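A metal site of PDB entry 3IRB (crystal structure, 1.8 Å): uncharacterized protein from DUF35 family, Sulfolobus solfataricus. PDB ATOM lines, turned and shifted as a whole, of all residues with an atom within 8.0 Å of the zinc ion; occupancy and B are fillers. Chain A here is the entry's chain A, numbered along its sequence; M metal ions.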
ATOM      1  N   LYS A  49     -25.419 -24.154 -23.894  1.00  0.00           N
ATOM      2  CA  LYS A  49     -26.853 -23.925 -24.021  1.00  0.00           C
ATOM      3  C   LYS A  49     -27.351 -24.451 -25.326  1.00  0.00           C
ATOM      4  O   LYS A  49     -26.939 -23.973 -26.387  1.00  0.00           O
ATOM      5  CB  LYS A  49     -27.195 -22.442 -23.870  1.00  0.00           C
ATOM      6  CG  LYS A  49     -28.671 -22.133 -24.023  1.00  0.00           C
ATOM      7  CD  LYS A  49     -28.984 -20.626 -23.916  1.00  0.00           C
ATOM      8  CE  LYS A  49     -30.484 -20.404 -23.759  1.00  0.00           C
ATOM      9  NZ  LYS A  49     -30.824 -18.971 -23.597  1.00  0.00           N
ATOM     10  N   CYS A  50     -28.242 -25.445 -25.269  1.00  0.00           N
ATOM     11  CA  CYS A  50     -28.861 -25.985 -26.470  1.00  0.00           C
ATOM     12  C   CYS A  50     -29.771 -24.936 -27.098  1.00  0.00           C
ATOM     13  O   CYS A  50     -30.628 -24.349 -26.446  1.00  0.00           O
ATOM     14  CB  CYS A  50     -29.673 -27.251 -26.166  1.00  0.00           C
ATOM     15  SG  CYS A  50     -30.521 -27.938 -27.548  1.00  0.00           S
ATOM     16  N   SER A  51     -29.574 -24.697 -28.381  1.00  0.00           N
ATOM     17  CA  SER A  51     -30.335 -23.678 -29.073  1.00  0.00           C
ATOM     18  C   SER A  51     -31.741 -24.153 -29.364  1.00  0.00           C
ATOM     19  O   SER A  51     -32.627 -23.354 -29.638  1.00  0.00           O
ATOM     20  CB  SER A  51     -29.640 -23.271 -30.365  1.00  0.00           C
ATOM     21  OG  SER A  51     -28.371 -22.721 -30.085  1.00  0.00           O
ATOM     22  N   LYS A  52     -31.940 -25.473 -29.346  1.00  0.00           N
ATOM     23  CA  LYS A  52     -33.248 -26.029 -29.711  1.00  0.00           C
ATOM     24  C   LYS A  52     -34.224 -26.043 -28.543  1.00  0.00           C
ATOM     25  O   LYS A  52     -35.408 -25.738 -28.739  1.00  0.00           O
ATOM     26  CB  LYS A  52     -33.132 -27.435 -30.279  1.00  0.00           C
ATOM     27  CG  LYS A  52     -34.396 -27.792 -31.055  1.00  0.00           C
ATOM     28  CD  LYS A  52     -34.236 -28.908 -32.047  1.00  0.00           C
ATOM     29  CE  LYS A  52     -35.425 -28.927 -33.018  1.00  0.00           C
ATOM     30  NZ  LYS A  52     -35.676 -30.287 -33.597  1.00  0.00           N
ATOM     31  N   CYS A  53     -33.736 -26.343 -27.338  1.00  0.00           N
ATOM     32  CA  CYS A  53     -34.622 -26.370 -26.148  1.00  0.00           C
ATOM     33  C   CYS A  53     -34.252 -25.334 -25.100  1.00  0.00           C
ATOM     34  O   CYS A  53     -34.986 -25.160 -24.106  1.00  0.00           O
ATOM     35  CB  CYS A  53     -34.605 -27.758 -25.519  1.00  0.00           C
ATOM     36  SG  CYS A  53     -33.000 -28.240 -24.801  1.00  0.00           S
ATOM     37  N   GLY A  54     -33.126 -24.652 -25.296  1.00  0.00           N
ATOM     38  CA  GLY A  54     -32.708 -23.637 -24.349  1.00  0.00           C
ATOM     39  C   GLY A  54     -32.141 -24.151 -23.032  1.00  0.00           C
ATOM     40  O   GLY A  54     -31.800 -23.352 -22.202  1.00  0.00           O
ATOM     41  N   ARG A  55     -32.058 -25.460 -22.813  1.00  0.00           N
ATOM     42  CA  ARG A  55     -31.437 -25.993 -21.590  1.00  0.00           C
ATOM     43  C   ARG A  55     -29.964 -25.580 -21.510  1.00  0.00           C
ATOM     44  O   ARG A  55     -29.242 -25.643 -22.525  1.00  0.00           O
ATOM     45  CB  ARG A  55     -31.525 -27.511 -21.584  1.00  0.00           C
ATOM     46  CG  ARG A  55     -32.931 -28.057 -21.363  1.00  0.00           C
ATOM     47  CD  ARG A  55     -32.900 -29.571 -21.339  1.00  0.00           C
ATOM     48  NE  ARG A  55     -34.188 -30.149 -20.995  1.00  0.00           N
ATOM     49  CZ  ARG A  55     -35.190 -30.335 -21.837  1.00  0.00           C
ATOM     50  NH1 ARG A  55     -35.092 -29.978 -23.122  1.00  0.00           N
ATOM     51  NH2 ARG A  55     -36.326 -30.868 -21.380  1.00  0.00           N
ATOM     52  N   ILE A  56     -29.527 -25.200 -20.300  1.00  0.00           N
ATOM     53  CA  ILE A  56     -28.143 -24.879 -20.029  1.00  0.00           C
ATOM     54  C   ILE A  56     -27.567 -26.012 -19.177  1.00  0.00           C
ATOM     55  O   ILE A  56     -28.181 -26.387 -18.215  1.00  0.00           O
ATOM     56  CB  ILE A  56     -28.019 -23.535 -19.298  1.00  0.00           C
ATOM     57  CG1 ILE A  56     -28.539 -22.389 -20.186  1.00  0.00           C
ATOM     58  CG2 ILE A  56     -26.573 -23.265 -18.970  1.00  0.00           C
ATOM     59  CD1 ILE A  56     -28.637 -21.029 -19.446  1.00  0.00           C
ATOM     60  N   PHE A  57     -26.431 -26.570 -19.605  1.00  0.00           N
ATOM     61  CA  PHE A  57     -25.837 -27.728 -18.962  1.00  0.00           C
ATOM     62  C   PHE A  57     -24.541 -27.332 -18.304  1.00  0.00           C
ATOM     63  O   PHE A  57     -23.733 -26.595 -18.888  1.00  0.00           O
ATOM     64  CB  PHE A  57     -25.506 -28.850 -19.948  1.00  0.00           C
ATOM     65  CG  PHE A  57     -26.696 -29.358 -20.705  1.00  0.00           C
ATOM     66  CD1 PHE A  57     -27.480 -30.383 -20.170  1.00  0.00           C
ATOM     67  CD2 PHE A  57     -27.067 -28.782 -21.910  1.00  0.00           C
ATOM     68  CE1 PHE A  57     -28.574 -30.865 -20.828  1.00  0.00           C
ATOM     69  CE2 PHE A  57     -28.181 -29.256 -22.581  1.00  0.00           C
ATOM     70  CZ  PHE A  57     -28.937 -30.306 -22.048  1.00  0.00           C
ATOM     71  N   TYR A  63     -23.431 -31.985 -26.860  1.00  0.00           N
ATOM     72  CA  TYR A  63     -24.607 -32.660 -27.424  1.00  0.00           C
ATOM     73  C   TYR A  63     -25.791 -32.592 -26.477  1.00  0.00           C
ATOM     74  O   TYR A  63     -25.623 -32.725 -25.262  1.00  0.00           O
ATOM     75  CB  TYR A  63     -24.279 -34.124 -27.675  1.00  0.00           C
ATOM     76  CG  TYR A  63     -25.332 -34.878 -28.507  1.00  0.00           C
ATOM     77  CD1 TYR A  63     -25.576 -34.518 -29.799  1.00  0.00           C
ATOM     78  CD2 TYR A  63     -26.024 -35.948 -27.983  1.00  0.00           C
ATOM     79  CE1 TYR A  63     -26.524 -35.200 -30.579  1.00  0.00           C
ATOM     80  CE2 TYR A  63     -26.969 -36.642 -28.735  1.00  0.00           C
ATOM     81  CZ  TYR A  63     -27.205 -36.262 -30.026  1.00  0.00           C
ATOM     82  OH  TYR A  63     -28.132 -36.933 -30.800  1.00  0.00           O
ATOM     83  N   CYS A  64     -26.988 -32.401 -27.019  1.00  0.00           N
ATOM     84  CA  CYS A  64     -28.193 -32.369 -26.204  1.00  0.00           C
ATOM     85  C   CYS A  64     -28.944 -33.672 -26.487  1.00  0.00           C
ATOM     86  O   CYS A  64     -29.449 -33.852 -27.574  1.00  0.00           O
ATOM     87  CB  CYS A  64     -29.094 -31.179 -26.558  1.00  0.00           C
ATOM     88  SG  CYS A  64     -30.666 -31.173 -25.575  1.00  0.00           S
ATOM     89  N   GLU A  65     -29.014 -34.570 -25.505  1.00  0.00           N
ATOM     90  CA  GLU A  65     -29.691 -35.857 -25.747  1.00  0.00           C
ATOM     91  C   GLU A  65     -31.237 -35.732 -25.725  1.00  0.00           C
ATOM     92  O   GLU A  65     -31.919 -36.622 -26.231  1.00  0.00           O
ATOM     93  CB  GLU A  65     -29.218 -36.935 -24.745  1.00  0.00           C
ATOM     94  CG  GLU A  65     -29.912 -38.316 -24.841  1.00  0.00           C
ATOM     95  CD  GLU A  65     -29.776 -39.054 -26.182  1.00  0.00           C
ATOM     96  OE1 GLU A  65     -29.074 -38.580 -27.111  1.00  0.00           O
ATOM     97  OE2 GLU A  65     -30.375 -40.139 -26.317  1.00  0.00           O
ATOM     98  N   HIS A  66     -31.760 -34.624 -25.188  1.00  0.00           N
ATOM     99  CA  HIS A  66     -33.197 -34.319 -25.252  1.00  0.00           C
ATOM    100  C   HIS A  66     -33.638 -34.021 -26.656  1.00  0.00           C
ATOM    101  O   HIS A  66     -34.662 -34.530 -27.099  1.00  0.00           O
ATOM    102  CB  HIS A  66     -33.544 -33.144 -24.333  1.00  0.00           C
ATOM    103  CG  HIS A  66     -33.308 -33.438 -22.892  1.00  0.00           C
ATOM    104  ND1 HIS A  66     -32.407 -32.737 -22.132  1.00  0.00           N
ATOM    105  CD2 HIS A  66     -33.830 -34.394 -22.089  1.00  0.00           C
ATOM    106  CE1 HIS A  66     -32.391 -33.234 -20.904  1.00  0.00           C
ATOM    107  NE2 HIS A  66     -33.247 -34.232 -20.849  1.00  0.00           N
ATOM    108  N   CYS A  67     -32.864 -33.189 -27.371  1.00  0.00           N
ATOM    109  CA  CYS A  67     -33.188 -32.771 -28.731  1.00  0.00           C
ATOM    110  C   CYS A  67     -32.494 -33.567 -29.830  1.00  0.00           C
ATOM    111  O   CYS A  67     -32.878 -33.441 -30.982  1.00  0.00           O
ATOM    112  CB  CYS A  67     -32.814 -31.299 -28.924  1.00  0.00           C
ATOM    113  SG  CYS A  67     -33.660 -30.162 -27.818  1.00  0.00           S
ATOM    114  N   PHE A  68     -31.472 -34.347 -29.489  1.00  0.00           N
ATOM    115  CA  PHE A  68     -30.626 -35.069 -30.455  1.00  0.00           C
ATOM    116  C   PHE A  68     -29.897 -34.147 -31.436  1.00  0.00           C
ATOM    117  O   PHE A  68     -29.933 -34.376 -32.637  1.00  0.00           O
ATOM    118  CB  PHE A  68     -31.441 -36.137 -31.228  1.00  0.00           C
ATOM    119  CG  PHE A  68     -32.275 -36.985 -30.339  1.00  0.00           C
ATOM    120  CD1 PHE A  68     -31.678 -37.850 -29.419  1.00  0.00           C
ATOM    121  CD2 PHE A  68     -33.659 -36.923 -30.382  1.00  0.00           C
ATOM    122  CE1 PHE A  68     -32.437 -38.625 -28.572  1.00  0.00           C
ATOM    123  CE2 PHE A  68     -34.432 -37.697 -29.537  1.00  0.00           C
ATOM    124  CZ  PHE A  68     -33.826 -38.556 -28.626  1.00  0.00           C
ATOM    125  N   VAL A  69     -29.287 -33.089 -30.902  1.00  0.00           N
ATOM    126  CA  VAL A  69     -28.586 -32.095 -31.693  1.00  0.00           C
ATOM    127  C   VAL A  69     -27.324 -31.648 -30.965  1.00  0.00           C
ATOM    128  O   VAL A  69     -27.233 -31.684 -29.712  1.00  0.00           O
ATOM    129  CB  VAL A  69     -29.442 -30.829 -31.971  1.00  0.00           C
ATOM    130  CG1 VAL A  69     -30.696 -31.171 -32.760  1.00  0.00           C
ATOM    131  CG2 VAL A  69     -29.774 -30.146 -30.692  1.00  0.00           C
ATOM    132  N   LYS A  70     -26.351 -31.246 -31.771  1.00  0.00           N
ATOM    133  CA  LYS A  70     -25.110 -30.656 -31.304  1.00  0.00           C
ATOM    134  C   LYS A  70     -25.386 -29.316 -30.584  1.00  0.00           C
ATOM    135  O   LYS A  70     -26.302 -28.553 -30.969  1.00  0.00           O
ATOM    136  CB  LYS A  70     -24.178 -30.411 -32.526  1.00  0.00           C
ATOM    137  CG  LYS A  70     -22.711 -30.676 -32.284  1.00  0.00           C
ATOM    138  CD  LYS A  70     -21.996 -29.526 -31.583  1.00  0.00           C
ATOM    139  CE  LYS A  70     -20.686 -29.984 -30.944  1.00  0.00           C
ATOM    140  N   ILE A  71     -24.612 -29.031 -29.538  1.00  0.00           N
ATOM    141  CA  ILE A  71     -24.652 -27.746 -28.840  1.00  0.00           C
ATOM    142  C   ILE A  71     -23.374 -26.971 -29.175  1.00  0.00           C
ATOM    143  O   ILE A  71     -22.272 -27.474 -28.990  1.00  0.00           O
ATOM    144  CB  ILE A  71     -24.694 -27.955 -27.308  1.00  0.00           C
ATOM    145  CG1 ILE A  71     -25.913 -28.814 -26.920  1.00  0.00           C
ATOM    146  CG2 ILE A  71     -24.701 -26.575 -26.544  1.00  0.00           C
ATOM    147  CD1 ILE A  71     -26.050 -29.067 -25.390  1.00  0.00           C
HETATM  148 ZN    ZN M   1     -31.958 -29.447 -26.453  1.00  0.00          ZN
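The guanidinium group of Arg 55 lies close to the side-chain sulfur of Cys 53. The side-chain sulfur (SG) of Cys 64 sits close to the backbone NH (N) of His 66 (3.6 Å). The backbone NH (N) of Cys 64 lies within hydrogen-bond range of the backbone carbonyl oxygen (O) of Val 69. SG of Cys 50 lies close to N of Lys 52 (3.4 Å). The backbone NH (N) of Cys 50 sits at hydrogen-bond distance from the backbone carbonyl oxygen (O) of Arg 55 (2.9 Å).
Within 4 Å of the zinc ion: Cys 50, Cys 53, Cys 64 and Cys 67. The nearest printed residue that does not touch the zinc ion is Lys 52 (4.5 Å).
The side-chain sulfur (SG) of Cys 53 is bound to the zinc ion (2.3 Å). SG of Cys 67 is bound to the zinc ion (2.3 Å). The zinc ion is bound by SG of Cys 64, 2.3 Å away. SG of Cys 50 binds the zinc ion (2.4 Å). The zinc ion has four donor atoms within binding distance.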
